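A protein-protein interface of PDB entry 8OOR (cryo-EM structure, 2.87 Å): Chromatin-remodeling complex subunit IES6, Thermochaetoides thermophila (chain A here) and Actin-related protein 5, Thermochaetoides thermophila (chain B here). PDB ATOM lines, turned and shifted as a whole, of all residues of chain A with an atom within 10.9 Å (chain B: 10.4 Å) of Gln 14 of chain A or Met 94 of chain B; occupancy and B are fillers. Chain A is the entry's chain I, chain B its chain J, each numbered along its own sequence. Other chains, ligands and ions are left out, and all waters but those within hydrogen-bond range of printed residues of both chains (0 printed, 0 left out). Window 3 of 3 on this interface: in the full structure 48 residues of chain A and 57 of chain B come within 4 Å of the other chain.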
ATOM      1  N   GLN A   7     -21.992 -16.039  -4.226  1.00  0.00           N
ATOM      2  CA  GLN A   7     -23.212 -15.395  -4.697  1.00  0.00           C
ATOM      3  C   GLN A   7     -23.271 -13.940  -4.253  1.00  0.00           C
ATOM      4  O   GLN A   7     -23.114 -13.637  -3.070  1.00  0.00           O
ATOM      5  CB  GLN A   7     -24.449 -16.147  -4.193  1.00  0.00           C
ATOM      6  CG  GLN A   7     -25.806 -15.508  -4.527  1.00  0.00           C
ATOM      7  CD  GLN A   7     -26.093 -15.341  -6.021  1.00  0.00           C
ATOM      8  OE1 GLN A   7     -25.204 -15.417  -6.869  1.00  0.00           O
ATOM      9  NE2 GLN A   7     -27.361 -15.110  -6.342  1.00  0.00           N
ATOM     10  N   SER A   8     -23.504 -13.045  -5.217  1.00  0.00           N
ATOM     11  CA  SER A   8     -23.421 -11.613  -4.943  1.00  0.00           C
ATOM     12  C   SER A   8     -24.404 -11.201  -3.856  1.00  0.00           C
ATOM     13  O   SER A   8     -24.095 -10.342  -3.022  1.00  0.00           O
ATOM     14  CB  SER A   8     -23.675 -10.817  -6.222  1.00  0.00           C
ATOM     15  OG  SER A   8     -24.970 -11.080  -6.734  1.00  0.00           O
ATOM     16  N   ALA A   9     -25.595 -11.802  -3.851  1.00  0.00           N
ATOM     17  CA  ALA A   9     -26.561 -11.507  -2.800  1.00  0.00           C
ATOM     18  C   ALA A   9     -26.022 -11.899  -1.432  1.00  0.00           C
ATOM     19  O   ALA A   9     -26.185 -11.159  -0.455  1.00  0.00           O
ATOM     20  CB  ALA A   9     -27.879 -12.226  -3.084  1.00  0.00           C
ATOM     21  N   GLN A  10     -25.360 -13.052  -1.345  1.00  0.00           N
ATOM     22  CA  GLN A  10     -24.752 -13.450  -0.083  1.00  0.00           C
ATOM     23  C   GLN A  10     -23.566 -12.560   0.262  1.00  0.00           C
ATOM     24  O   GLN A  10     -23.374 -12.197   1.428  1.00  0.00           O
ATOM     25  CB  GLN A  10     -24.335 -14.919  -0.146  1.00  0.00           C
ATOM     26  CG  GLN A  10     -23.887 -15.515   1.183  1.00  0.00           C
ATOM     27  CD  GLN A  10     -22.421 -15.261   1.488  1.00  0.00           C
ATOM     28  OE1 GLN A  10     -21.679 -14.752   0.649  1.00  0.00           O
ATOM     29  NE2 GLN A  10     -22.000 -15.617   2.695  1.00  0.00           N
ATOM     30  N   ALA A  11     -22.762 -12.197  -0.738  1.00  0.00           N
ATOM     31  CA  ALA A  11     -21.675 -11.252  -0.504  1.00  0.00           C
ATOM     32  C   ALA A  11     -22.200  -9.895  -0.057  1.00  0.00           C
ATOM     33  O   ALA A  11     -21.628  -9.265   0.840  1.00  0.00           O
ATOM     34  CB  ALA A  11     -20.829 -11.107  -1.768  1.00  0.00           C
ATOM     35  N   ALA A  12     -23.293  -9.431  -0.664  1.00  0.00           N
ATOM     36  CA  ALA A  12     -23.926  -8.202  -0.200  1.00  0.00           C
ATOM     37  C   ALA A  12     -24.458  -8.351   1.217  1.00  0.00           C
ATOM     38  O   ALA A  12     -24.334  -7.433   2.034  1.00  0.00           O
ATOM     39  CB  ALA A  12     -25.051  -7.797  -1.151  1.00  0.00           C
ATOM     40  N   HIS A  13     -25.041  -9.507   1.531  1.00  0.00           N
ATOM     41  CA  HIS A  13     -25.492  -9.758   2.893  1.00  0.00           C
ATOM     42  C   HIS A  13     -24.331  -9.728   3.878  1.00  0.00           C
ATOM     43  O   HIS A  13     -24.453  -9.163   4.971  1.00  0.00           O
ATOM     44  CB  HIS A  13     -26.225 -11.094   2.963  1.00  0.00           C
ATOM     45  CG  HIS A  13     -26.848 -11.367   4.295  1.00  0.00           C
ATOM     46  ND1 HIS A  13     -26.151 -11.925   5.345  1.00  0.00           N
ATOM     47  CD2 HIS A  13     -28.108 -11.164   4.746  1.00  0.00           C
ATOM     48  CE1 HIS A  13     -26.954 -12.052   6.385  1.00  0.00           C
ATOM     49  NE2 HIS A  13     -28.148 -11.599   6.048  1.00  0.00           N
ATOM     50  N   GLN A  14     -23.203 -10.339   3.519  1.00  0.00           N
ATOM     51  CA  GLN A  14     -21.999 -10.207   4.334  1.00  0.00           C
ATOM     52  C   GLN A  14     -21.594  -8.748   4.482  1.00  0.00           C
ATOM     53  O   GLN A  14     -21.234  -8.298   5.574  1.00  0.00           O
ATOM     54  CB  GLN A  14     -20.855 -11.018   3.732  1.00  0.00           C
ATOM     55  CG  GLN A  14     -21.003 -12.510   3.904  1.00  0.00           C
ATOM     56  CD  GLN A  14     -19.738 -13.258   3.550  1.00  0.00           C
ATOM     57  OE1 GLN A  14     -18.891 -12.754   2.814  1.00  0.00           O
ATOM     58  NE2 GLN A  14     -19.600 -14.469   4.075  1.00  0.00           N
ATOM     59  N   ALA A  15     -21.624  -7.999   3.382  1.00  0.00           N
ATOM     60  CA  ALA A  15     -21.294  -6.582   3.450  1.00  0.00           C
ATOM     61  C   ALA A  15     -22.221  -5.829   4.395  1.00  0.00           C
ATOM     62  O   ALA A  15     -21.770  -4.973   5.163  1.00  0.00           O
ATOM     63  CB  ALA A  15     -21.353  -5.969   2.051  1.00  0.00           C
ATOM     64  N   LEU A  16     -23.517  -6.139   4.366  1.00  0.00           N
ATOM     65  CA  LEU A  16     -24.447  -5.487   5.281  1.00  0.00           C
ATOM     66  C   LEU A  16     -24.132  -5.781   6.743  1.00  0.00           C
ATOM     67  O   LEU A  16     -23.982  -4.857   7.547  1.00  0.00           O
ATOM     68  CB  LEU A  16     -25.876  -5.903   4.954  1.00  0.00           C
ATOM     69  CG  LEU A  16     -26.418  -5.262   3.682  1.00  0.00           C
ATOM     70  CD1 LEU A  16     -27.696  -5.948   3.240  1.00  0.00           C
ATOM     71  CD2 LEU A  16     -26.648  -3.782   3.910  1.00  0.00           C
ATOM     72  N   VAL A  17     -24.016  -7.057   7.111  1.00  0.00           N
ATOM     73  CA  VAL A  17     -23.736  -7.377   8.510  1.00  0.00           C
ATOM     74  C   VAL A  17     -22.382  -6.827   8.935  1.00  0.00           C
ATOM     75  O   VAL A  17     -22.210  -6.380  10.075  1.00  0.00           O
ATOM     76  CB  VAL A  17     -23.838  -8.892   8.765  1.00  0.00           C
ATOM     77  CG1 VAL A  17     -25.270  -9.350   8.595  1.00  0.00           C
ATOM     78  CG2 VAL A  17     -22.916  -9.664   7.857  1.00  0.00           C
ATOM     79  N   GLU A  18     -21.400  -6.847   8.035  1.00  0.00           N
ATOM     80  CA  GLU A  18     -20.120  -6.242   8.373  1.00  0.00           C
ATOM     81  C   GLU A  18     -20.230  -4.733   8.524  1.00  0.00           C
ATOM     82  O   GLU A  18     -19.546  -4.145   9.369  1.00  0.00           O
ATOM     83  CB  GLU A  18     -19.067  -6.609   7.330  1.00  0.00           C
ATOM     84  CG  GLU A  18     -18.617  -8.062   7.409  1.00  0.00           C
ATOM     85  CD  GLU A  18     -17.666  -8.328   8.569  1.00  0.00           C
ATOM     86  OE1 GLU A  18     -17.584  -7.487   9.490  1.00  0.00           O
ATOM     87  OE2 GLU A  18     -16.997  -9.383   8.563  1.00  0.00           O
ATOM     88  N   GLN A  19     -21.088  -4.094   7.732  1.00  0.00           N
ATOM     89  CA  GLN A  19     -21.316  -2.664   7.893  1.00  0.00           C
ATOM     90  C   GLN A  19     -22.131  -2.364   9.144  1.00  0.00           C
ATOM     91  O   GLN A  19     -21.941  -1.316   9.771  1.00  0.00           O
ATOM     92  CB  GLN A  19     -22.008  -2.114   6.650  1.00  0.00           C
ATOM     93  CG  GLN A  19     -22.386  -0.657   6.723  1.00  0.00           C
ATOM     94  CD  GLN A  19     -22.852  -0.127   5.383  1.00  0.00           C
ATOM     95  OE1 GLN A  19     -22.720  -0.799   4.361  1.00  0.00           O
ATOM     96  NE2 GLN A  19     -23.393   1.082   5.379  1.00  0.00           N
ATOM     97  N   LEU A  20     -23.024  -3.275   9.528  1.00  0.00           N
ATOM     98  CA  LEU A  20     -23.878  -3.080  10.693  1.00  0.00           C
ATOM     99  C   LEU A  20     -23.215  -3.489  11.999  1.00  0.00           C
ATOM    100  O   LEU A  20     -23.599  -2.986  13.057  1.00  0.00           O
ATOM    101  CB  LEU A  20     -25.178  -3.857  10.523  1.00  0.00           C
ATOM    102  CG  LEU A  20     -26.107  -3.307   9.449  1.00  0.00           C
ATOM    103  CD1 LEU A  20     -27.171  -4.318   9.120  1.00  0.00           C
ATOM    104  CD2 LEU A  20     -26.728  -2.029   9.920  1.00  0.00           C
ATOM    105  N   ASP A  21     -22.261  -4.413  11.960  1.00  0.00           N
ATOM    106  CA  ASP A  21     -21.716  -4.975  13.189  1.00  0.00           C
ATOM    107  C   ASP A  21     -21.120  -3.896  14.084  1.00  0.00           C
ATOM    108  O   ASP A  21     -20.396  -3.012  13.622  1.00  0.00           O
ATOM    109  CB  ASP A  21     -20.657  -6.027  12.878  1.00  0.00           C
ATOM    110  CG  ASP A  21     -19.974  -6.540  14.129  1.00  0.00           C
ATOM    111  OD1 ASP A  21     -20.686  -6.895  15.089  1.00  0.00           O
ATOM    112  OD2 ASP A  21     -18.728  -6.574  14.163  1.00  0.00           O
ATOM    113  N   LEU A  22     -21.458  -3.966  15.370  1.00  0.00           N
ATOM    114  CA  LEU A  22     -20.809  -3.145  16.383  1.00  0.00           C
ATOM    115  C   LEU A  22     -19.478  -3.720  16.831  1.00  0.00           C
ATOM    116  O   LEU A  22     -18.580  -2.966  17.215  1.00  0.00           O
ATOM    117  CB  LEU A  22     -21.701  -3.024  17.615  1.00  0.00           C
ATOM    118  CG  LEU A  22     -22.952  -2.165  17.593  1.00  0.00           C
ATOM    119  CD1 LEU A  22     -23.706  -2.429  18.873  1.00  0.00           C
ATOM    120  CD2 LEU A  22     -22.575  -0.701  17.472  1.00  0.00           C
ATOM    121  N   SER A  24     -16.878  -5.137  15.477  1.00  0.00           N
ATOM    122  CA  SER A  24     -15.685  -4.666  14.783  1.00  0.00           C
ATOM    123  C   SER A  24     -15.343  -3.214  15.080  1.00  0.00           C
ATOM    124  O   SER A  24     -14.315  -2.737  14.590  1.00  0.00           O
ATOM    125  CB  SER A  24     -15.855  -4.843  13.274  1.00  0.00           C
ATOM    126  OG  SER A  24     -17.051  -4.234  12.824  1.00  0.00           O
ATOM    127  N   TYR B  89     -23.943 -13.036  18.175  1.00  0.00           N
ATOM    128  CA  TYR B  89     -23.711 -14.452  17.935  1.00  0.00           C
ATOM    129  C   TYR B  89     -22.326 -14.642  17.339  1.00  0.00           C
ATOM    130  O   TYR B  89     -21.755 -13.726  16.743  1.00  0.00           O
ATOM    131  CB  TYR B  89     -24.784 -15.045  17.025  1.00  0.00           C
ATOM    132  CG  TYR B  89     -24.936 -14.353  15.696  1.00  0.00           C
ATOM    133  CD1 TYR B  89     -24.107 -14.659  14.632  1.00  0.00           C
ATOM    134  CD2 TYR B  89     -25.910 -13.394  15.507  1.00  0.00           C
ATOM    135  CE1 TYR B  89     -24.245 -14.024  13.420  1.00  0.00           C
ATOM    136  CE2 TYR B  89     -26.060 -12.762  14.297  1.00  0.00           C
ATOM    137  CZ  TYR B  89     -25.224 -13.078  13.260  1.00  0.00           C
ATOM    138  OH  TYR B  89     -25.382 -12.451  12.049  1.00  0.00           O
ATOM    139  N   ARG B  90     -21.802 -15.855  17.499  1.00  0.00           N
ATOM    140  CA  ARG B  90     -20.638 -16.326  16.755  1.00  0.00           C
ATOM    141  C   ARG B  90     -21.082 -16.970  15.448  1.00  0.00           C
ATOM    142  O   ARG B  90     -21.754 -18.004  15.455  1.00  0.00           O
ATOM    143  CB  ARG B  90     -19.830 -17.316  17.590  1.00  0.00           C
ATOM    144  CG  ARG B  90     -18.432 -17.566  17.062  1.00  0.00           C
ATOM    145  CD  ARG B  90     -17.462 -16.466  17.425  1.00  0.00           C
ATOM    146  NE  ARG B  90     -16.167 -16.684  16.794  1.00  0.00           N
ATOM    147  CZ  ARG B  90     -15.066 -16.003  17.082  1.00  0.00           C
ATOM    148  NH1 ARG B  90     -15.081 -14.999  17.942  1.00  0.00           N
ATOM    149  NH2 ARG B  90     -13.928 -16.325  16.475  1.00  0.00           N
ATOM    150  N   ASP B  91     -20.707 -16.360  14.328  1.00  0.00           N
ATOM    151  CA  ASP B  91     -20.991 -16.941  13.023  1.00  0.00           C
ATOM    152  C   ASP B  91     -20.069 -18.130  12.782  1.00  0.00           C
ATOM    153  O   ASP B  91     -18.842 -17.988  12.797  1.00  0.00           O
ATOM    154  CB  ASP B  91     -20.814 -15.896  11.928  1.00  0.00           C
ATOM    155  CG  ASP B  91     -21.285 -16.384  10.570  1.00  0.00           C
ATOM    156  OD1 ASP B  91     -20.615 -17.258   9.981  1.00  0.00           O
ATOM    157  OD2 ASP B  91     -22.323 -15.889  10.087  1.00  0.00           O
ATOM    158  N   ARG B  92     -20.663 -19.304  12.562  1.00  0.00           N
ATOM    159  CA  ARG B  92     -19.875 -20.526  12.435  1.00  0.00           C
ATOM    160  C   ARG B  92     -19.061 -20.553  11.148  1.00  0.00           C
ATOM    161  O   ARG B  92     -18.013 -21.207  11.095  1.00  0.00           O
ATOM    162  CB  ARG B  92     -20.794 -21.746  12.492  1.00  0.00           C
ATOM    163  CG  ARG B  92     -21.715 -21.793  13.698  1.00  0.00           C
ATOM    164  CD  ARG B  92     -20.961 -21.621  15.005  1.00  0.00           C
ATOM    165  NE  ARG B  92     -20.008 -22.699  15.233  1.00  0.00           N
ATOM    166  CZ  ARG B  92     -19.346 -22.886  16.367  1.00  0.00           C
ATOM    167  NH1 ARG B  92     -19.508 -22.080  17.403  1.00  0.00           N
ATOM    168  NH2 ARG B  92     -18.502 -23.909  16.464  1.00  0.00           N
ATOM    169  N   LYS B  93     -19.508 -19.843  10.114  1.00  0.00           N
ATOM    170  CA  LYS B  93     -18.843 -19.887   8.816  1.00  0.00           C
ATOM    171  C   LYS B  93     -17.799 -18.793   8.649  1.00  0.00           C
ATOM    172  O   LYS B  93     -16.705 -19.056   8.137  1.00  0.00           O
ATOM    173  CB  LYS B  93     -19.886 -19.777   7.705  1.00  0.00           C
ATOM    174  CG  LYS B  93     -20.867 -20.930   7.679  1.00  0.00           C
ATOM    175  CD  LYS B  93     -21.831 -20.812   6.515  1.00  0.00           C
ATOM    176  CE  LYS B  93     -22.816 -21.970   6.501  1.00  0.00           C
ATOM    177  NZ  LYS B  93     -23.760 -21.895   5.348  1.00  0.00           N
ATOM    178  N   MET B  94     -18.110 -17.569   9.063  1.00  0.00           N
ATOM    179  CA  MET B  94     -17.125 -16.497   9.048  1.00  0.00           C
ATOM    180  C   MET B  94     -16.168 -16.568  10.230  1.00  0.00           C
ATOM    181  O   MET B  94     -15.133 -15.896  10.210  1.00  0.00           O
ATOM    182  CB  MET B  94     -17.827 -15.139   9.005  1.00  0.00           C
ATOM    183  CG  MET B  94     -18.730 -14.979   7.789  1.00  0.00           C
ATOM    184  SD  MET B  94     -19.490 -13.355   7.628  1.00  0.00           S
ATOM    185  CE  MET B  94     -18.101 -12.382   7.055  1.00  0.00           C
ATOM    186  N   GLY B  95     -16.493 -17.356  11.252  1.00  0.00           N
ATOM    187  CA  GLY B  95     -15.561 -17.613  12.330  1.00  0.00           C
ATOM    188  C   GLY B  95     -15.384 -16.476  13.306  1.00  0.00           C
ATOM    189  O   GLY B  95     -14.397 -16.453  14.043  1.00  0.00           O
ATOM    190  N   LYS B  96     -16.322 -15.534  13.340  1.00  0.00           N
ATOM    191  CA  LYS B  96     -16.130 -14.270  14.029  1.00  0.00           C
ATOM    192  C   LYS B  96     -17.425 -13.896  14.732  1.00  0.00           C
ATOM    193  O   LYS B  96     -18.513 -14.324  14.344  1.00  0.00           O
ATOM    194  CB  LYS B  96     -15.700 -13.169  13.053  1.00  0.00           C
ATOM    195  CG  LYS B  96     -16.793 -12.776  12.084  1.00  0.00           C
ATOM    196  CD  LYS B  96     -16.272 -11.890  10.968  1.00  0.00           C
ATOM    197  CE  LYS B  96     -15.731 -10.577  11.491  1.00  0.00           C
ATOM    198  NZ  LYS B  96     -15.255  -9.712  10.378  1.00  0.00           N
ATOM    199  N   THR B  97     -17.294 -13.088  15.776  1.00  0.00           N
ATOM    200  CA  THR B  97     -18.456 -12.569  16.477  1.00  0.00           C
ATOM    201  C   THR B  97     -19.106 -11.451  15.676  1.00  0.00           C
ATOM    202  O   THR B  97     -18.428 -10.637  15.048  1.00  0.00           O
ATOM    203  CB  THR B  97     -18.068 -12.066  17.865  1.00  0.00           C
ATOM    204  OG1 THR B  97     -17.454 -13.129  18.600  1.00  0.00           O
ATOM    205  CG2 THR B  97     -19.295 -11.612  18.621  1.00  0.00           C
ATOM    206  N   PHE B  98     -20.432 -11.434  15.685  1.00  0.00           N
ATOM    207  CA  PHE B  98     -21.214 -10.294  15.238  1.00  0.00           C
ATOM    208  C   PHE B  98     -22.035  -9.776  16.405  1.00  0.00           C
ATOM    209  O   PHE B  98     -22.478 -10.550  17.258  1.00  0.00           O
ATOM    210  CB  PHE B  98     -22.119 -10.671  14.078  1.00  0.00           C
ATOM    211  CG  PHE B  98     -21.389 -10.850  12.791  1.00  0.00           C
ATOM    212  CD1 PHE B  98     -20.783 -12.051  12.488  1.00  0.00           C
ATOM    213  CD2 PHE B  98     -21.309  -9.818  11.880  1.00  0.00           C
ATOM    214  CE1 PHE B  98     -20.110 -12.218  11.299  1.00  0.00           C
ATOM    215  CE2 PHE B  98     -20.638  -9.979  10.689  1.00  0.00           C
ATOM    216  CZ  PHE B  98     -20.036 -11.180  10.400  1.00  0.00           C
ATOM    217  N   PHE B 100     -25.078  -6.568  17.333  1.00  0.00           N
ATOM    218  CA  PHE B 100     -26.057  -5.659  16.766  1.00  0.00           C
ATOM    219  C   PHE B 100     -26.851  -5.062  17.911  1.00  0.00           C
ATOM    220  O   PHE B 100     -26.965  -5.662  18.980  1.00  0.00           O
ATOM    221  CB  PHE B 100     -26.997  -6.361  15.790  1.00  0.00           C
ATOM    222  CG  PHE B 100     -26.297  -7.075  14.678  1.00  0.00           C
ATOM    223  CD1 PHE B 100     -25.794  -6.379  13.603  1.00  0.00           C
ATOM    224  CD2 PHE B 100     -26.134  -8.442  14.717  1.00  0.00           C
ATOM    225  CE1 PHE B 100     -25.158  -7.034  12.582  1.00  0.00           C
ATOM    226  CE2 PHE B 100     -25.494  -9.098  13.699  1.00  0.00           C
ATOM    227  CZ  PHE B 100     -25.005  -8.392  12.632  1.00  0.00           C
ATOM    228  N   TYR B 106     -32.599  -6.722  12.615  1.00  0.00           N
ATOM    229  CA  TYR B 106     -33.715  -7.033  11.718  1.00  0.00           C
ATOM    230  C   TYR B 106     -35.044  -7.153  12.459  1.00  0.00           C
ATOM    231  O   TYR B 106     -35.880  -7.993  12.129  1.00  0.00           O
ATOM    232  CB  TYR B 106     -33.440  -8.296  10.910  1.00  0.00           C
ATOM    233  CG  TYR B 106     -32.200  -8.212  10.070  1.00  0.00           C
ATOM    234  CD1 TYR B 106     -30.964  -8.521  10.600  1.00  0.00           C
ATOM    235  CD2 TYR B 106     -32.266  -7.818   8.747  1.00  0.00           C
ATOM    236  CE1 TYR B 106     -29.828  -8.441   9.838  1.00  0.00           C
ATOM    237  CE2 TYR B 106     -31.139  -7.736   7.977  1.00  0.00           C
ATOM    238  CZ  TYR B 106     -29.921  -8.047   8.528  1.00  0.00           C
ATOM    239  OH  TYR B 106     -28.782  -7.971   7.762  1.00  0.00           O
ATOM    240  N   ALA B 111     -29.860 -12.043  10.226  1.00  0.00           N
ATOM    241  CA  ALA B 111     -31.167 -12.658  10.043  1.00  0.00           C
ATOM    242  C   ALA B 111     -31.342 -13.866  10.956  1.00  0.00           C
ATOM    243  O   ALA B 111     -32.286 -14.640  10.801  1.00  0.00           O
ATOM    244  CB  ALA B 111     -31.364 -13.056   8.600  1.00  0.00           C
ATOM    245  N   ARG B 112     -30.408 -14.039  11.893  1.00  0.00           N
ATOM    246  CA  ARG B 112     -30.561 -15.080  12.900  1.00  0.00           C
ATOM    247  C   ARG B 112     -31.538 -14.678  13.997  1.00  0.00           C
ATOM    248  O   ARG B 112     -32.178 -15.550  14.599  1.00  0.00           O
ATOM    249  CB  ARG B 112     -29.207 -15.404  13.523  1.00  0.00           C
ATOM    250  CG  ARG B 112     -28.188 -15.906  12.530  1.00  0.00           C
ATOM    251  CD  ARG B 112     -26.947 -16.412  13.229  1.00  0.00           C
ATOM    252  NE  ARG B 112     -25.899 -16.743  12.271  1.00  0.00           N
ATOM    253  CZ  ARG B 112     -25.816 -17.887  11.605  1.00  0.00           C
ATOM    254  NH1 ARG B 112     -26.710 -18.849  11.770  1.00  0.00           N
ATOM    255  NH2 ARG B 112     -24.818 -18.065  10.745  1.00  0.00           N
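Of chain B, only Met 94 comes within 4 Å of Gln 14 of chain A. Met 94 of chain B touches just these residues of chain A: Gln 14 (3.7 Å) and Glu 18 (3.5 Å). No residue of chain B comes within 4 Å of Gln 10 of chain A. No residue of chain B comes within 4 Å of Ala 11 of chain A. No residue of chain B comes within 4 Å of Ala 15 of chain A. No residue of chain A comes within 4 Å of Asp 91 of chain B. Of chain A, only Glu 18 comes within 4 Å of Lys 96 of chain B. Of the printed residues of chain A, Phe 98 of chain B touches Val 17, Glu 18 and Asp 21. Of the printed residues of chain B, Leu 20 of chain A touches Phe 100 (3.8 Å). Of the printed residues of chain A, Phe 100 of chain B touches Val 17, Leu 20 and Asp 21. Thr 97 of chain B touches none of the printed residues of chain A. Ser 24 of chain A touches none of the printed residues of chain B.
NE2 of Gln 14 of chain A sits at hydrogen-bond distance from SD of Met 94 of chain B (3.7 Å). The side-chain amino group (NZ) of Lys 96 of chain B lies within salt-bridge range of the side-chain carboxylate (OE2) of Glu 18 of chain A (2.5 Å).
Hydrophobic or aromatic side chains of chain A that line the printed part of chain B: Val 17 and Leu 20. Hydrophobic or aromatic side chains of chain B that line the printed part of chain A: Met 94, Phe 98, Phe 100 and Tyr 106. Along chain B the printed residues that touch a printed residue of chain A span positions 94 to 106. Among the printed residues, Asp or Glu carboxylates within 4 Å of a Lys or Arg side-chain nitrogen of the other chain: Glu 18 of chain A with Lys 96 of chain B (2.5 Å).
Val 17 of chain A touches Phe 98 of chain B (CG2 to CE2, 3.6 Å). O of Val 17 of chain A touches CE1 of Phe 100 of chain B (3.9 Å). Val 17 of chain A touches Tyr 106 of chain B (CG1 to OH, 3.9 Å). Glu 18 of chain A touches Met 94 of chain B. Phe 98 of chain B touches Glu 18 of chain A (CZ to OE2, 3.98 Å). CE1 of Phe 100 of chain B touches CB of Leu 20 of chain A, at 3.8 Å. Phe 98 of chain B touches Asp 21 of chain A (C to OD1, 3.4 Å). CE1 of Phe 100 of chain B touches N of Asp 21 of chain A (3.96 Å).
N of Asp 91 of chain B is in hydrogen-bond range of O of Lys 96 of chain B, at 3.0 Å. NE2 of Gln 10 of chain A lies close to NE2 of Gln 14 of chain A. The backbone carbonyl oxygen (O) of Tyr 89 of chain B is in hydrogen-bond range of the backbone NH (N) of Phe 98 of chain B. N of Ser 24 of chain A is in hydrogen-bond range of OD2 of Asp 21 of chain A, 2.7 Å away. N of Met 94 of chain B lies within hydrogen-bond range of OD1 of Asp 91 of chain B.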
